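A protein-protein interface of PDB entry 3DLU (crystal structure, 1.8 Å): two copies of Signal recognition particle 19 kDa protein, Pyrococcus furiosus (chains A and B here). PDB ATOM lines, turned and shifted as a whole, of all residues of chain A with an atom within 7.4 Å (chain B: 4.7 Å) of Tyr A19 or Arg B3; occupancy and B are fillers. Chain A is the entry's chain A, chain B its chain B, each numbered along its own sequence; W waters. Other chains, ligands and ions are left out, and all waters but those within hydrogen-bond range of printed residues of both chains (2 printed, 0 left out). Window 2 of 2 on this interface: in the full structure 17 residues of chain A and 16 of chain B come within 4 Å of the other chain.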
ATOM      1  N   TRP A   7      -5.901  -2.961  -8.688  1.00  0.00           N
ATOM      2  CA  TRP A   7      -5.302  -4.152  -9.254  1.00  0.00           C
ATOM      3  C   TRP A   7      -5.605  -5.274  -8.236  1.00  0.00           C
ATOM      4  O   TRP A   7      -5.283  -5.131  -7.053  1.00  0.00           O
ATOM      5  CB  TRP A   7      -3.797  -3.887  -9.462  1.00  0.00           C
ATOM      6  CG  TRP A   7      -2.998  -5.075  -9.892  1.00  0.00           C
ATOM      7  CD1 TRP A   7      -3.286  -5.931 -10.915  1.00  0.00           C
ATOM      8  CD2 TRP A   7      -1.752  -5.514  -9.337  1.00  0.00           C
ATOM      9  NE1 TRP A   7      -2.303  -6.900 -11.014  1.00  0.00           N
ATOM     10  CE2 TRP A   7      -1.351  -6.660 -10.057  1.00  0.00           C
ATOM     11  CE3 TRP A   7      -0.939  -5.055  -8.295  1.00  0.00           C
ATOM     12  CZ2 TRP A   7      -0.167  -7.355  -9.767  1.00  0.00           C
ATOM     13  CZ3 TRP A   7       0.238  -5.749  -8.006  1.00  0.00           C
ATOM     14  CH2 TRP A   7       0.604  -6.887  -8.742  1.00  0.00           C
ATOM     15  N   SER A   9      -4.501  -7.982  -7.162  1.00  0.00           N
ATOM     16  CA  SER A   9      -3.449  -8.458  -6.244  1.00  0.00           C
ATOM     17  C   SER A   9      -3.241  -7.564  -5.025  1.00  0.00           C
ATOM     18  O   SER A   9      -2.762  -8.023  -3.985  1.00  0.00           O
ATOM     19  CB  SER A   9      -2.119  -8.654  -6.990  1.00  0.00           C
ATOM     20  OG  SER A   9      -2.272  -9.676  -7.961  1.00  0.00           O
ATOM     21  N   GLU A  10      -3.609  -6.291  -5.149  1.00  0.00           N
ATOM     22  CA  GLU A  10      -3.484  -5.346  -4.036  1.00  0.00           C
ATOM     23  C   GLU A  10      -4.262  -5.791  -2.797  1.00  0.00           C
ATOM     24  O   GLU A  10      -3.891  -5.454  -1.684  1.00  0.00           O
ATOM     25  CB  GLU A  10      -3.939  -3.940  -4.466  1.00  0.00           C
ATOM     26  CG  GLU A  10      -2.988  -3.289  -5.493  1.00  0.00           C
ATOM     27  CD  GLU A  10      -3.599  -2.064  -6.170  1.00  0.00           C
ATOM     28  OE1 GLU A  10      -4.833  -1.894  -6.110  1.00  0.00           O
ATOM     29  OE2 GLU A  10      -2.845  -1.277  -6.776  1.00  0.00           O
ATOM     30  N   ARG A  14      -3.612 -14.133  -0.432  1.00  0.00           N
ATOM     31  CA  ARG A  14      -2.684 -15.202  -0.806  1.00  0.00           C
ATOM     32  C   ARG A  14      -1.274 -14.683  -1.108  1.00  0.00           C
ATOM     33  O   ARG A  14      -0.312 -15.442  -1.106  1.00  0.00           O
ATOM     34  CB  ARG A  14      -3.229 -15.997  -1.995  1.00  0.00           C
ATOM     35  CG  ARG A  14      -4.488 -16.789  -1.664  1.00  0.00           C
ATOM     36  CD  ARG A  14      -4.791 -17.856  -2.701  1.00  0.00           C
ATOM     37  NE  ARG A  14      -3.756 -18.888  -2.766  1.00  0.00           N
ATOM     38  CZ  ARG A  14      -3.556 -19.817  -1.834  1.00  0.00           C
ATOM     39  NH1 ARG A  14      -4.306 -19.845  -0.742  1.00  0.00           N
ATOM     40  NH2 ARG A  14      -2.594 -20.719  -1.989  1.00  0.00           N
ATOM     41  N   LEU A  15      -1.149 -13.388  -1.359  1.00  0.00           N
ATOM     42  CA  LEU A  15       0.141 -12.820  -1.773  1.00  0.00           C
ATOM     43  C   LEU A  15       0.832 -12.103  -0.638  1.00  0.00           C
ATOM     44  O   LEU A  15       0.183 -11.546   0.238  1.00  0.00           O
ATOM     45  CB  LEU A  15      -0.066 -11.824  -2.922  1.00  0.00           C
ATOM     46  CG  LEU A  15      -0.804 -12.386  -4.125  1.00  0.00           C
ATOM     47  CD1 LEU A  15      -1.009 -11.290  -5.192  1.00  0.00           C
ATOM     48  CD2 LEU A  15      -0.058 -13.588  -4.686  1.00  0.00           C
ATOM     49  N   SER A  16       2.160 -12.087  -0.670  1.00  0.00           N
ATOM     50  CA  SER A  16       2.918 -11.250   0.251  1.00  0.00           C
ATOM     51  C   SER A  16       2.865  -9.809  -0.251  1.00  0.00           C
ATOM     52  O   SER A  16       2.479  -9.563  -1.394  1.00  0.00           O
ATOM     53  CB  SER A  16       4.373 -11.716   0.309  1.00  0.00           C
ATOM     54  OG  SER A  16       4.965 -11.649  -0.980  1.00  0.00           O
ATOM     55  N   ARG A  17       3.260  -8.862   0.593  1.00  0.00           N
ATOM     56  CA  ARG A  17       3.362  -7.477   0.154  1.00  0.00           C
ATOM     57  C   ARG A  17       4.360  -7.344  -0.994  1.00  0.00           C
ATOM     58  O   ARG A  17       4.133  -6.567  -1.920  1.00  0.00           O
ATOM     59  CB  ARG A  17       3.691  -6.542   1.327  1.00  0.00           C
ATOM     60  CG  ARG A  17       2.508  -6.360   2.287  1.00  0.00           C
ATOM     61  CD  ARG A  17       2.882  -5.645   3.591  1.00  0.00           C
ATOM     62  NE  ARG A  17       1.715  -5.455   4.458  1.00  0.00           N
ATOM     63  CZ  ARG A  17       0.845  -4.455   4.326  1.00  0.00           C
ATOM     64  NH1 ARG A  17       1.014  -3.558   3.365  1.00  0.00           N
ATOM     65  NH2 ARG A  17      -0.199  -4.351   5.146  1.00  0.00           N
ATOM     66  N   LYS A  18       5.445  -8.121  -0.951  1.00  0.00           N
ATOM     67  CA  LYS A  18       6.440  -8.115  -2.031  1.00  0.00           C
ATOM     68  C   LYS A  18       5.830  -8.461  -3.389  1.00  0.00           C
ATOM     69  O   LYS A  18       6.277  -7.956  -4.425  1.00  0.00           O
ATOM     70  CB  LYS A  18       7.598  -9.072  -1.727  1.00  0.00           C
ATOM     71  N   TYR A  19       4.816  -9.325  -3.391  1.00  0.00           N
ATOM     72  CA  TYR A  19       4.145  -9.677  -4.641  1.00  0.00           C
ATOM     73  C   TYR A  19       2.931  -8.814  -4.962  1.00  0.00           C
ATOM     74  O   TYR A  19       2.183  -9.129  -5.882  1.00  0.00           O
ATOM     75  CB  TYR A  19       3.787 -11.166  -4.699  1.00  0.00           C
ATOM     76  CG  TYR A  19       4.996 -12.000  -5.026  1.00  0.00           C
ATOM     77  CD1 TYR A  19       5.922 -12.327  -4.045  1.00  0.00           C
ATOM     78  CD2 TYR A  19       5.236 -12.424  -6.326  1.00  0.00           C
ATOM     79  CE1 TYR A  19       7.048 -13.076  -4.343  1.00  0.00           C
ATOM     80  CE2 TYR A  19       6.355 -13.172  -6.637  1.00  0.00           C
ATOM     81  CZ  TYR A  19       7.259 -13.495  -5.644  1.00  0.00           C
ATOM     82  OH  TYR A  19       8.373 -14.241  -5.954  1.00  0.00           O
ATOM     83  N   GLY A  20       2.741  -7.733  -4.221  1.00  0.00           N
ATOM     84  CA  GLY A  20       1.758  -6.746  -4.635  1.00  0.00           C
ATOM     85  C   GLY A  20       0.674  -6.392  -3.641  1.00  0.00           C
ATOM     86  O   GLY A  20       0.006  -5.384  -3.821  1.00  0.00           O
ATOM     87  N   ARG A  21       0.492  -7.194  -2.592  1.00  0.00           N
ATOM     88  CA  ARG A  21      -0.557  -6.898  -1.623  1.00  0.00           C
ATOM     89  C   ARG A  21      -0.293  -5.609  -0.841  1.00  0.00           C
ATOM     90  O   ARG A  21       0.819  -5.381  -0.334  1.00  0.00           O
ATOM     91  CB  ARG A  21      -0.811  -8.074  -0.657  1.00  0.00           C
ATOM     92  CG  ARG A  21      -1.850  -7.714   0.411  1.00  0.00           C
ATOM     93  CD  ARG A  21      -2.350  -8.913   1.209  1.00  0.00           C
ATOM     94  NE  ARG A  21      -1.252  -9.725   1.703  1.00  0.00           N
ATOM     95  CZ  ARG A  21      -0.527  -9.437   2.784  1.00  0.00           C
ATOM     96  NH1 ARG A  21      -0.775  -8.349   3.501  1.00  0.00           N
ATOM     97  NH2 ARG A  21       0.463 -10.244   3.142  1.00  0.00           N
ATOM     98  N   ILE A  22      -1.320  -4.769  -0.786  1.00  0.00           N
ATOM     99  CA  ILE A  22      -1.281  -3.487  -0.098  1.00  0.00           C
ATOM    100  C   ILE A  22      -1.899  -3.600   1.281  1.00  0.00           C
ATOM    101  O   ILE A  22      -1.322  -3.158   2.270  1.00  0.00           O
ATOM    102  CB  ILE A  22      -2.100  -2.407  -0.861  1.00  0.00           C
ATOM    103  CG1 ILE A  22      -1.562  -2.205  -2.273  1.00  0.00           C
ATOM    104  CG2 ILE A  22      -2.110  -1.095  -0.094  1.00  0.00           C
ATOM    105  CD1 ILE A  22      -1.939  -0.874  -2.880  1.00  0.00           C
ATOM    106  N   GLY B   2       9.348  -3.919  -4.531  1.00  0.00           N
ATOM    107  CA  GLY B   2       7.987  -4.416  -4.504  1.00  0.00           C
ATOM    108  C   GLY B   2       7.360  -4.457  -5.885  1.00  0.00           C
ATOM    109  O   GLY B   2       7.875  -3.877  -6.839  1.00  0.00           O
ATOM    110  N   ARG B   3       6.241  -5.159  -5.984  1.00  0.00           N
ATOM    111  CA  ARG B   3       5.506  -5.282  -7.230  1.00  0.00           C
ATOM    112  C   ARG B   3       4.273  -4.381  -7.127  1.00  0.00           C
ATOM    113  O   ARG B   3       3.613  -4.358  -6.106  1.00  0.00           O
ATOM    114  CB  ARG B   3       5.118  -6.753  -7.430  1.00  0.00           C
ATOM    115  CG  ARG B   3       4.507  -7.065  -8.763  1.00  0.00           C
ATOM    116  CD  ARG B   3       4.216  -8.549  -8.891  1.00  0.00           C
ATOM    117  NE  ARG B   3       5.430  -9.332  -9.095  1.00  0.00           N
ATOM    118  CZ  ARG B   3       5.436 -10.575  -9.574  1.00  0.00           C
ATOM    119  NH1 ARG B   3       4.295 -11.161  -9.896  1.00  0.00           N
ATOM    120  NH2 ARG B   3       6.578 -11.223  -9.744  1.00  0.00           N
ATOM    121  N   PHE B   4       3.981  -3.606  -8.167  1.00  0.00           N
ATOM    122  CA  PHE B   4       2.811  -2.719  -8.134  1.00  0.00           C
ATOM    123  C   PHE B   4       2.363  -2.388  -9.546  1.00  0.00           C
ATOM    124  O   PHE B   4       3.094  -2.647 -10.511  1.00  0.00           O
ATOM    125  CB  PHE B   4       3.089  -1.429  -7.344  1.00  0.00           C
ATOM    126  CG  PHE B   4       4.311  -0.687  -7.808  1.00  0.00           C
ATOM    127  CD1 PHE B   4       5.523  -0.838  -7.147  1.00  0.00           C
ATOM    128  CD2 PHE B   4       4.246   0.174  -8.893  1.00  0.00           C
ATOM    129  CE1 PHE B   4       6.658  -0.155  -7.574  1.00  0.00           C
ATOM    130  CE2 PHE B   4       5.381   0.868  -9.335  1.00  0.00           C
ATOM    131  CZ  PHE B   4       6.589   0.699  -8.669  1.00  0.00           C
ATOM    132  N   ILE B  49       6.383  -7.139 -15.376  1.00  0.00           N
ATOM    133  CA  ILE B  49       5.682  -8.388 -15.138  1.00  0.00           C
ATOM    134  C   ILE B  49       4.510  -8.562 -16.110  1.00  0.00           C
ATOM    135  O   ILE B  49       4.305  -9.643 -16.663  1.00  0.00           O
ATOM    136  CB  ILE B  49       5.194  -8.441 -13.675  1.00  0.00           C
ATOM    137  CG1 ILE B  49       6.396  -8.346 -12.729  1.00  0.00           C
ATOM    138  CG2 ILE B  49       4.414  -9.703 -13.391  1.00  0.00           C
ATOM    139  CD1 ILE B  49       7.518  -9.298 -13.091  1.00  0.00           C
ATOM    140  N   VAL B  74       2.273  -3.887 -14.907  1.00  0.00           N
ATOM    141  CA  VAL B  74       2.702  -4.382 -13.601  1.00  0.00           C
ATOM    142  C   VAL B  74       4.224  -4.440 -13.602  1.00  0.00           C
ATOM    143  O   VAL B  74       4.824  -5.036 -14.511  1.00  0.00           O
ATOM    144  CB  VAL B  74       2.124  -5.777 -13.265  1.00  0.00           C
ATOM    145  CG1 VAL B  74       2.646  -6.238 -11.896  1.00  0.00           C
ATOM    146  CG2 VAL B  74       0.575  -5.741 -13.287  1.00  0.00           C
ATOM    147  N   LEU B  75       4.828  -3.810 -12.592  1.00  0.00           N
ATOM    148  CA  LEU B  75       6.286  -3.687 -12.492  1.00  0.00           C
ATOM    149  C   LEU B  75       6.811  -4.121 -11.123  1.00  0.00           C
ATOM    150  O   LEU B  75       6.093  -4.073 -10.120  1.00  0.00           O
ATOM    151  CB  LEU B  75       6.718  -2.224 -12.692  1.00  0.00           C
ATOM    152  CG  LEU B  75       6.488  -1.493 -14.006  1.00  0.00           C
ATOM    153  CD1 LEU B  75       6.967  -0.037 -13.884  1.00  0.00           C
ATOM    154  CD2 LEU B  75       7.202  -2.206 -15.141  1.00  0.00           C
ATOM    155  N   GLU B  76       8.084  -4.501 -11.083  1.00  0.00           N
ATOM    156  CA  GLU B  76       8.783  -4.624  -9.805  1.00  0.00           C
ATOM    157  C   GLU B  76       9.889  -3.580  -9.731  1.00  0.00           C
ATOM    158  O   GLU B  76      10.652  -3.406 -10.688  1.00  0.00           O
ATOM    159  CB  GLU B  76       9.354  -6.034  -9.618  1.00  0.00           C
ATOM    160  CG  GLU B  76       8.319  -7.131  -9.720  1.00  0.00           C
ATOM    161  CD  GLU B  76       8.895  -8.506  -9.441  1.00  0.00           C
ATOM    162  OE1 GLU B  76      10.092  -8.725  -9.723  1.00  0.00           O
ATOM    163  OE2 GLU B  76       8.144  -9.371  -8.947  1.00  0.00           O
HETATM  164  O   HOH W   1       1.879 -10.811  -7.966  1.00  0.00           O
HETATM  165  O   HOH W   2       4.886  -4.148  -3.234  1.00  0.00           O
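No position is printed for both chains.
Of the 7 pairs that touch across the chains among the printed residues, none has its exchanged pair printed and touching as well.
Water W1 bridges O of Tyr A19 (2.7 Å) and NH1 of Arg B3 (3.1 Å).
Water W2 bridges the backbone carbonyl oxygen (O) of Arg A17 (2.9 Å) and the backbone carbonyl oxygen (O) of Arg B3 (3.1 Å).
Tyr A19 touches just one residue of chain B: Arg B3 (3.7 Å).
Of the printed residues of chain A, Gly B2 touches Lys A18.
Of chain A, only Trp A7, Lys A18, Tyr A19 and Gly A20 come within 4 Å of Arg B3.
Of the printed residues of chain A, Phe B4 touches Trp A7 (3.98 Å).
The nearest residue of chain A that does not touch Arg B3 is Arg A17 (4.8 Å).
The nearest printed residue of chain B that does not touch Gly A20 is Phe B4 (5.2 Å).
Of the 7 printed residues of chain B, 4 touch a printed residue of chain A.
Among the printed residues, 7 pairs touch across the chains.
Among the printed residues, no Asp or Glu carboxylate lies within 4 Å of a Lys or Arg side-chain nitrogen of the other chain.
N of Trp A7 sits at hydrogen-bond distance from OE1 of Glu A10 (3.0 Å).
OG of Ser A16 sits close to N of Tyr A19 (3.4 Å).
The side-chain carboxylate of Glu B76 lies within salt-bridge range of the guanidinium group of Arg B3 (2.6 Å).
The backbone NH (N) of Phe B4 is in hydrogen-bond range of the backbone carbonyl oxygen (O) of Leu B75, 2.9 Å away.
O of Val B74 sits at hydrogen-bond distance from N of Ile B49, at 2.8 Å.
CG of Arg B3 touches CH2 of Trp A7, 3.9 Å away.
Trp A7 touches Phe B4 (CZ3 to CA, 3.98 Å).
CZ2 of Trp A7 touches CG1 of Val B74, 3.7 Å away.
Lys A18 touches Gly B2.
Arg B3 touches Tyr A19 (NH2 to CE2, 3.7 Å).
Gly A20 touches Arg B3 (CA to O, 3.4 Å).
The backbone carbonyl oxygen (O) of Lys A18 lies within hydrogen-bond range of the backbone NH (N) of Arg B3.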
